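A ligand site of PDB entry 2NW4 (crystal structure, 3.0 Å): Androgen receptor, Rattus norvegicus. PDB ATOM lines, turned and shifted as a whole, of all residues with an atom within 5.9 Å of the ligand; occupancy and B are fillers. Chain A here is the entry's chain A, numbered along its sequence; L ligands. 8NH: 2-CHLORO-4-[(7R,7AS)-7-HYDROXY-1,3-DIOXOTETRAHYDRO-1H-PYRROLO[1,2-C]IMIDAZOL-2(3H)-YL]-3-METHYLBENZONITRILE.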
ATOM      1  N   LEU A  42      13.565  -8.740 -31.643  1.00  0.00           N
ATOM      2  CA  LEU A  42      15.014  -8.858 -31.804  1.00  0.00           C
ATOM      3  C   LEU A  42      15.700  -7.809 -32.667  1.00  0.00           C
ATOM      4  O   LEU A  42      16.800  -7.359 -32.333  1.00  0.00           O
ATOM      5  CB  LEU A  42      15.370 -10.246 -32.292  1.00  0.00           C
ATOM      6  CG  LEU A  42      15.208 -11.129 -31.067  1.00  0.00           C
ATOM      7  CD1 LEU A  42      14.144 -12.132 -31.370  1.00  0.00           C
ATOM      8  CD2 LEU A  42      16.534 -11.762 -30.677  1.00  0.00           C
ATOM      9  N   LEU A  45      16.030  -5.444 -30.047  1.00  0.00           N
ATOM     10  CA  LEU A  45      16.970  -5.862 -29.005  1.00  0.00           C
ATOM     11  C   LEU A  45      18.387  -5.635 -29.537  1.00  0.00           C
ATOM     12  O   LEU A  45      19.217  -5.047 -28.841  1.00  0.00           O
ATOM     13  CB  LEU A  45      16.787  -7.342 -28.635  1.00  0.00           C
ATOM     14  CG  LEU A  45      15.801  -7.725 -27.524  1.00  0.00           C
ATOM     15  CD1 LEU A  45      15.816  -9.217 -27.329  1.00  0.00           C
ATOM     16  CD2 LEU A  45      16.186  -7.049 -26.237  1.00  0.00           C
ATOM     17  N   ASN A  46      18.647  -6.104 -30.754  1.00  0.00           N
ATOM     18  CA  ASN A  46      19.942  -5.967 -31.417  1.00  0.00           C
ATOM     19  C   ASN A  46      20.348  -4.486 -31.495  1.00  0.00           C
ATOM     20  O   ASN A  46      21.516  -4.134 -31.273  1.00  0.00           O
ATOM     21  CB  ASN A  46      19.905  -6.563 -32.840  1.00  0.00           C
ATOM     22  CG  ASN A  46      19.677  -8.080 -32.840  1.00  0.00           C
ATOM     23  OD1 ASN A  46      19.475  -8.676 -33.907  1.00  0.00           O
ATOM     24  ND2 ASN A  46      19.722  -8.710 -31.672  1.00  0.00           N
ATOM     25  N   GLU A  47      19.387  -3.630 -31.829  1.00  0.00           N
ATOM     26  CA  GLU A  47      19.622  -2.193 -31.930  1.00  0.00           C
ATOM     27  C   GLU A  47      19.984  -1.633 -30.559  1.00  0.00           C
ATOM     28  O   GLU A  47      20.742  -0.682 -30.436  1.00  0.00           O
ATOM     29  CB  GLU A  47      18.372  -1.485 -32.445  1.00  0.00           C
ATOM     30  CG  GLU A  47      18.515   0.031 -32.497  1.00  0.00           C
ATOM     31  CD  GLU A  47      19.564   0.475 -33.514  1.00  0.00           C
ATOM     32  OE1 GLU A  47      20.003  -0.360 -34.330  1.00  0.00           O
ATOM     33  OE2 GLU A  47      19.940   1.667 -33.496  1.00  0.00           O
ATOM     34  N   LEU A  48      19.400  -2.234 -29.525  1.00  0.00           N
ATOM     35  CA  LEU A  48      19.676  -1.819 -28.162  1.00  0.00           C
ATOM     36  C   LEU A  48      21.075  -2.320 -27.846  1.00  0.00           C
ATOM     37  O   LEU A  48      21.841  -1.634 -27.186  1.00  0.00           O
ATOM     38  CB  LEU A  48      18.655  -2.428 -27.189  1.00  0.00           C
ATOM     39  CG  LEU A  48      18.678  -1.880 -25.753  1.00  0.00           C
ATOM     40  CD1 LEU A  48      18.957  -0.399 -25.770  1.00  0.00           C
ATOM     41  CD2 LEU A  48      17.357  -2.136 -25.082  1.00  0.00           C
ATOM     42  N   GLY A  49      21.386  -3.523 -28.315  1.00  0.00           N
ATOM     43  CA  GLY A  49      22.710  -4.066 -28.086  1.00  0.00           C
ATOM     44  C   GLY A  49      23.680  -3.011 -28.554  1.00  0.00           C
ATOM     45  O   GLY A  49      24.490  -2.522 -27.789  1.00  0.00           O
ATOM     46  N   GLN A  52      23.676   0.156 -26.421  1.00  0.00           N
ATOM     47  CA  GLN A  52      24.297  -0.101 -25.142  1.00  0.00           C
ATOM     48  C   GLN A  52      25.799  -0.316 -25.268  1.00  0.00           C
ATOM     49  O   GLN A  52      26.553   0.076 -24.383  1.00  0.00           O
ATOM     50  CB  GLN A  52      23.623  -1.298 -24.458  1.00  0.00           C
ATOM     51  CG  GLN A  52      22.504  -0.852 -23.525  1.00  0.00           C
ATOM     52  CD  GLN A  52      23.009   0.018 -22.370  1.00  0.00           C
ATOM     53  OE1 GLN A  52      22.254   0.824 -21.823  1.00  0.00           O
ATOM     54  NE2 GLN A  52      24.275  -0.140 -21.999  1.00  0.00           N
ATOM     55  N   TRP A  82      30.684  -7.544 -22.891  1.00  0.00           N
ATOM     56  CA  TRP A  82      29.533  -6.667 -23.014  1.00  0.00           C
ATOM     57  C   TRP A  82      28.166  -7.308 -22.753  1.00  0.00           C
ATOM     58  O   TRP A  82      27.324  -6.685 -22.110  1.00  0.00           O
ATOM     59  CB  TRP A  82      29.579  -5.898 -24.336  1.00  0.00           C
ATOM     60  CG  TRP A  82      28.952  -6.542 -25.499  1.00  0.00           C
ATOM     61  CD1 TRP A  82      29.246  -7.782 -26.016  1.00  0.00           C
ATOM     62  CD2 TRP A  82      27.959  -5.972 -26.344  1.00  0.00           C
ATOM     63  NE1 TRP A  82      28.482  -8.010 -27.153  1.00  0.00           N
ATOM     64  CE2 TRP A  82      27.691  -6.910 -27.370  1.00  0.00           C
ATOM     65  CE3 TRP A  82      27.271  -4.760 -26.339  1.00  0.00           C
ATOM     66  CZ2 TRP A  82      26.761  -6.673 -28.380  1.00  0.00           C
ATOM     67  CZ3 TRP A  82      26.351  -4.527 -27.339  1.00  0.00           C
ATOM     68  CH2 TRP A  82      26.100  -5.482 -28.348  1.00  0.00           C
ATOM     69  N   MET A  83      27.951  -8.531 -23.191  1.00  0.00           N
ATOM     70  CA  MET A  83      26.676  -9.216 -22.956  1.00  0.00           C
ATOM     71  C   MET A  83      26.459  -9.265 -21.450  1.00  0.00           C
ATOM     72  O   MET A  83      25.475  -8.741 -20.944  1.00  0.00           O
ATOM     73  CB  MET A  83      26.716 -10.632 -23.511  1.00  0.00           C
ATOM     74  CG  MET A  83      25.377 -11.330 -23.565  1.00  0.00           C
ATOM     75  SD  MET A  83      24.280 -10.436 -24.658  1.00  0.00           S
ATOM     76  CE  MET A  83      25.303 -10.375 -26.178  1.00  0.00           C
ATOM     77  N   MET A  86      25.752  -5.903 -20.093  1.00  0.00           N
ATOM     78  CA  MET A  86      24.408  -5.494 -20.479  1.00  0.00           C
ATOM     79  C   MET A  86      23.374  -6.245 -19.644  1.00  0.00           C
ATOM     80  O   MET A  86      22.343  -5.689 -19.259  1.00  0.00           O
ATOM     81  CB  MET A  86      24.139  -5.758 -21.969  1.00  0.00           C
ATOM     82  CG  MET A  86      24.720  -4.725 -22.903  1.00  0.00           C
ATOM     83  SD  MET A  86      23.878  -4.719 -24.487  1.00  0.00           S
ATOM     84  CE  MET A  86      24.012  -6.452 -24.899  1.00  0.00           C
ATOM     85  N   VAL A  87      23.642  -7.527 -19.388  1.00  0.00           N
ATOM     86  CA  VAL A  87      22.752  -8.345 -18.604  1.00  0.00           C
ATOM     87  C   VAL A  87      22.691  -7.873 -17.161  1.00  0.00           C
ATOM     88  O   VAL A  87      21.620  -7.692 -16.616  1.00  0.00           O
ATOM     89  CB  VAL A  87      23.196  -9.812 -18.577  1.00  0.00           C
ATOM     90  CG1 VAL A  87      22.515 -10.529 -17.424  1.00  0.00           C
ATOM     91  CG2 VAL A  87      22.865 -10.485 -19.899  1.00  0.00           C
ATOM     92  N   MET A  90      21.020  -4.450 -16.828  1.00  0.00           N
ATOM     93  CA  MET A  90      19.630  -4.664 -17.195  1.00  0.00           C
ATOM     94  C   MET A  90      18.871  -5.315 -16.048  1.00  0.00           C
ATOM     95  O   MET A  90      17.751  -4.921 -15.742  1.00  0.00           O
ATOM     96  CB  MET A  90      19.537  -5.521 -18.451  1.00  0.00           C
ATOM     97  CG  MET A  90      18.129  -5.660 -19.028  1.00  0.00           C
ATOM     98  SD  MET A  90      16.975  -6.773 -18.132  1.00  0.00           S
ATOM     99  CE  MET A  90      17.037  -8.220 -19.133  1.00  0.00           C
ATOM    100  N   ARG A  93      18.144  -2.586 -13.575  1.00  0.00           N
ATOM    101  CA  ARG A  93      17.101  -1.656 -13.966  1.00  0.00           C
ATOM    102  C   ARG A  93      15.772  -2.296 -13.678  1.00  0.00           C
ATOM    103  O   ARG A  93      14.876  -1.679 -13.108  1.00  0.00           O
ATOM    104  CB  ARG A  93      17.155  -1.349 -15.451  1.00  0.00           C
ATOM    105  CG  ARG A  93      18.155  -0.306 -15.823  1.00  0.00           C
ATOM    106  CD  ARG A  93      17.795   0.310 -17.159  1.00  0.00           C
ATOM    107  NE  ARG A  93      17.884  -0.655 -18.262  1.00  0.00           N
ATOM    108  CZ  ARG A  93      18.995  -1.243 -18.649  1.00  0.00           C
ATOM    109  NH1 ARG A  93      20.152  -0.989 -18.036  1.00  0.00           N
ATOM    110  NH2 ARG A  93      18.968  -2.106 -19.653  1.00  0.00           N
ATOM    111  N   PHE A 105      14.348  -3.713 -20.339  1.00  0.00           N
ATOM    112  CA  PHE A 105      15.477  -3.524 -21.236  1.00  0.00           C
ATOM    113  C   PHE A 105      15.750  -2.046 -21.394  1.00  0.00           C
ATOM    114  O   PHE A 105      16.888  -1.596 -21.237  1.00  0.00           O
ATOM    115  CB  PHE A 105      15.211  -4.164 -22.593  1.00  0.00           C
ATOM    116  CG  PHE A 105      15.406  -5.643 -22.587  1.00  0.00           C
ATOM    117  CD1 PHE A 105      16.681  -6.179 -22.467  1.00  0.00           C
ATOM    118  CD2 PHE A 105      14.314  -6.507 -22.652  1.00  0.00           C
ATOM    119  CE1 PHE A 105      16.874  -7.542 -22.399  1.00  0.00           C
ATOM    120  CE2 PHE A 105      14.487  -7.879 -22.589  1.00  0.00           C
ATOM    121  CZ  PHE A 105      15.772  -8.406 -22.465  1.00  0.00           C
ATOM    122  N   ALA A 106      14.716  -1.292 -21.740  1.00  0.00           N
ATOM    123  CA  ALA A 106      14.806   0.146 -21.900  1.00  0.00           C
ATOM    124  C   ALA A 106      13.426   0.659 -21.570  1.00  0.00           C
ATOM    125  O   ALA A 106      12.494  -0.125 -21.386  1.00  0.00           O
ATOM    126  CB  ALA A 106      15.166   0.501 -23.314  1.00  0.00           C
ATOM    127  N   MET A 121      13.170 -16.160 -26.595  1.00  0.00           N
ATOM    128  CA  MET A 121      14.205 -16.220 -25.575  1.00  0.00           C
ATOM    129  C   MET A 121      13.582 -16.501 -24.217  1.00  0.00           C
ATOM    130  O   MET A 121      14.204 -16.278 -23.183  1.00  0.00           O
ATOM    131  CB  MET A 121      14.963 -14.897 -25.511  1.00  0.00           C
ATOM    132  CG  MET A 121      15.404 -14.338 -26.842  1.00  0.00           C
ATOM    133  SD  MET A 121      16.169 -12.733 -26.527  1.00  0.00           S
ATOM    134  CE  MET A 121      17.647 -13.295 -25.712  1.00  0.00           C
ATOM    135  N   MET A 128      17.407 -14.335 -16.823  1.00  0.00           N
ATOM    136  CA  MET A 128      17.701 -12.936 -16.612  1.00  0.00           C
ATOM    137  C   MET A 128      16.816 -12.321 -15.529  1.00  0.00           C
ATOM    138  O   MET A 128      17.289 -11.534 -14.705  1.00  0.00           O
ATOM    139  CB  MET A 128      17.555 -12.169 -17.923  1.00  0.00           C
ATOM    140  CG  MET A 128      18.364 -12.777 -19.055  1.00  0.00           C
ATOM    141  SD  MET A 128      18.114 -11.979 -20.633  1.00  0.00           S
ATOM    142  CE  MET A 128      19.284 -10.645 -20.456  1.00  0.00           C
ATOM    143  N   LEU A 214      23.176 -16.478 -23.935  1.00  0.00           N
ATOM    144  CA  LEU A 214      22.754 -15.349 -24.742  1.00  0.00           C
ATOM    145  C   LEU A 214      23.677 -15.244 -25.938  1.00  0.00           C
ATOM    146  O   LEU A 214      23.254 -14.890 -27.043  1.00  0.00           O
ATOM    147  CB  LEU A 214      22.829 -14.037 -23.956  1.00  0.00           C
ATOM    148  CG  LEU A 214      21.666 -13.716 -23.030  1.00  0.00           C
ATOM    149  CD1 LEU A 214      21.981 -12.476 -22.254  1.00  0.00           C
ATOM    150  CD2 LEU A 214      20.393 -13.532 -23.830  1.00  0.00           C
ATOM    151  N   PHE A 217      22.626 -17.820 -28.467  1.00  0.00           N
ATOM    152  CA  PHE A 217      21.387 -17.412 -29.119  1.00  0.00           C
ATOM    153  C   PHE A 217      21.660 -16.366 -30.178  1.00  0.00           C
ATOM    154  O   PHE A 217      21.282 -16.535 -31.336  1.00  0.00           O
ATOM    155  CB  PHE A 217      20.394 -16.875 -28.086  1.00  0.00           C
ATOM    156  CG  PHE A 217      19.056 -16.494 -28.663  1.00  0.00           C
ATOM    157  CD1 PHE A 217      18.860 -15.248 -29.264  1.00  0.00           C
ATOM    158  CD2 PHE A 217      17.981 -17.390 -28.609  1.00  0.00           C
ATOM    159  CE1 PHE A 217      17.608 -14.900 -29.811  1.00  0.00           C
ATOM    160  CE2 PHE A 217      16.729 -17.045 -29.147  1.00  0.00           C
ATOM    161  CZ  PHE A 217      16.543 -15.800 -29.748  1.00  0.00           C
ATOM    162  N   THR A 218      22.325 -15.300 -29.778  1.00  0.00           N
ATOM    163  CA  THR A 218      22.636 -14.217 -30.703  1.00  0.00           C
ATOM    164  C   THR A 218      23.446 -14.707 -31.898  1.00  0.00           C
ATOM    165  O   THR A 218      23.128 -14.377 -33.054  1.00  0.00           O
ATOM    166  CB  THR A 218      23.414 -13.088 -29.979  1.00  0.00           C
ATOM    167  OG1 THR A 218      22.575 -12.511 -28.969  1.00  0.00           O
ATOM    168  CG2 THR A 218      23.853 -12.007 -30.987  1.00  0.00           C
ATOM    169  N   LEU A 221      21.494 -16.654 -34.216  1.00  0.00           N
ATOM    170  CA  LEU A 221      20.580 -15.665 -34.775  1.00  0.00           C
ATOM    171  C   LEU A 221      21.212 -14.861 -35.902  1.00  0.00           C
ATOM    172  O   LEU A 221      20.523 -14.504 -36.865  1.00  0.00           O
ATOM    173  CB  LEU A 221      20.078 -14.725 -33.684  1.00  0.00           C
ATOM    174  CG  LEU A 221      18.997 -13.748 -34.179  1.00  0.00           C
ATOM    175  CD1 LEU A 221      17.997 -14.512 -35.063  1.00  0.00           C
ATOM    176  CD2 LEU A 221      18.296 -13.082 -33.004  1.00  0.00           C
ATOM    177  N   PHE A 232      20.719  -6.688 -37.790  1.00  0.00           N
ATOM    178  CA  PHE A 232      21.989  -6.667 -37.088  1.00  0.00           C
ATOM    179  C   PHE A 232      22.828  -5.472 -37.499  1.00  0.00           C
ATOM    180  O   PHE A 232      23.148  -5.299 -38.672  1.00  0.00           O
ATOM    181  CB  PHE A 232      22.800  -7.937 -37.346  1.00  0.00           C
ATOM    182  CG  PHE A 232      22.543  -9.039 -36.369  1.00  0.00           C
ATOM    183  CD1 PHE A 232      21.352  -9.749 -36.390  1.00  0.00           C
ATOM    184  CD2 PHE A 232      23.484  -9.355 -35.407  1.00  0.00           C
ATOM    185  CE1 PHE A 232      21.105 -10.755 -35.474  1.00  0.00           C
ATOM    186  CE2 PHE A 232      23.246 -10.355 -34.477  1.00  0.00           C
ATOM    187  CZ  PHE A 232      22.056 -11.062 -34.508  1.00  0.00           C
ATOM    188  N   MET A 236      27.572  -4.453 -33.743  1.00  0.00           N
ATOM    189  CA  MET A 236      27.180  -5.679 -33.071  1.00  0.00           C
ATOM    190  C   MET A 236      27.547  -6.966 -33.842  1.00  0.00           C
ATOM    191  O   MET A 236      28.171  -7.872 -33.275  1.00  0.00           O
ATOM    192  CB  MET A 236      25.677  -5.644 -32.796  1.00  0.00           C
ATOM    193  CG  MET A 236      25.208  -6.620 -31.755  1.00  0.00           C
ATOM    194  SD  MET A 236      23.436  -6.493 -31.467  1.00  0.00           S
ATOM    195  CE  MET A 236      22.908  -8.112 -31.953  1.00  0.00           C
HETATM  196 CL1  8NH L   1      20.305  -6.676 -21.351  1.00  0.00          CL
HETATM  197  C2  8NH L   1      20.403  -6.530 -23.156  1.00  0.00           C
HETATM  198  C3  8NH L   1      20.525  -7.694 -23.942  1.00  0.00           C
HETATM  199  C4  8NH L   1      20.483  -7.578 -25.336  1.00  0.00           C
HETATM  200  C5  8NH L   1      20.392  -6.345 -25.994  1.00  0.00           C
HETATM  201  C7  8NH L   1      20.381  -5.197 -25.223  1.00  0.00           C
HETATM  202  C9  8NH L   1      20.333  -5.275 -23.815  1.00  0.00           C
HETATM  203  C10 8NH L   1      20.065  -4.037 -23.147  1.00  0.00           C
HETATM  204  N11 8NH L   1      19.742  -3.059 -22.641  1.00  0.00           N
HETATM  205  N12 8NH L   1      20.558  -8.655 -26.128  1.00  0.00           N
HETATM  206  C13 8NH L   1      19.577  -9.568 -26.326  1.00  0.00           C
HETATM  207  N14 8NH L   1      20.047 -10.536 -27.100  1.00  0.00           N
HETATM  208  C15 8NH L   1      21.346 -10.225 -27.626  1.00  0.00           C
HETATM  209  C17 8NH L   1      20.940  -9.969 -29.053  1.00  0.00           C
HETATM  210  C19 8NH L   1      19.833 -11.008 -29.342  1.00  0.00           C
HETATM  211  C22 8NH L   1      19.274 -11.371 -27.964  1.00  0.00           C
HETATM  212  O25 8NH L   1      20.394  -8.649 -29.026  1.00  0.00           O
HETATM  213  C27 8NH L   1      21.559  -8.839 -26.991  1.00  0.00           C
HETATM  214  O28 8NH L   1      22.468  -8.049 -27.250  1.00  0.00           O
HETATM  215  O29 8NH L   1      18.431  -9.490 -25.880  1.00  0.00           O
HETATM  216  C30 8NH L   1      20.716  -9.032 -23.320  1.00  0.00           C
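An oxygen (O25) of the ligand sits at hydrogen-bond distance from the side-chain amide nitrogen (ND2) of Asn 46 (2.7 Å). The guanidinium group (NH2) of Arg 93 sits at hydrogen-bond distance from a nitrogen (N11) of the ligand.
ND2 of Asn 46 sits close to O of Leu 42 (3.3 Å). The backbone carbonyl oxygen of Leu 214 lies within hydrogen-bond range of the side-chain hydroxyl of Thr 218 (3.1 Å). NH2 of Arg 93 sits at hydrogen-bond distance from O of Phe 105, at 2.7 Å.
Merely in contact with the ligand: Thr 218 (2.9 Å), Leu 45 (3.0 Å), Met 86 (3.1 Å), Met 90 (3.2 Å), Met 121 (3.4 Å), Leu 48 (3.5 Å), Phe 105 (3.5 Å), Met 128 (3.6 Å), Leu 42 (3.6 Å), Gln 52 (3.6 Å), Gly 49 (3.7 Å), Met 83 (3.8 Å), Leu 214 (3.8 Å), Met 236 (3.9 Å) and Val 87 (3.96 Å). Hydrophobic or aromatic side chains that line the ligand: Leu 42, Leu 45, Leu 48, Met 83, Met 86, Met 90, Phe 105, Met 121, Met 128, Leu 214 and Met 236. The nearest printed residue that does not touch the ligand is Phe 217 (4.1 Å).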
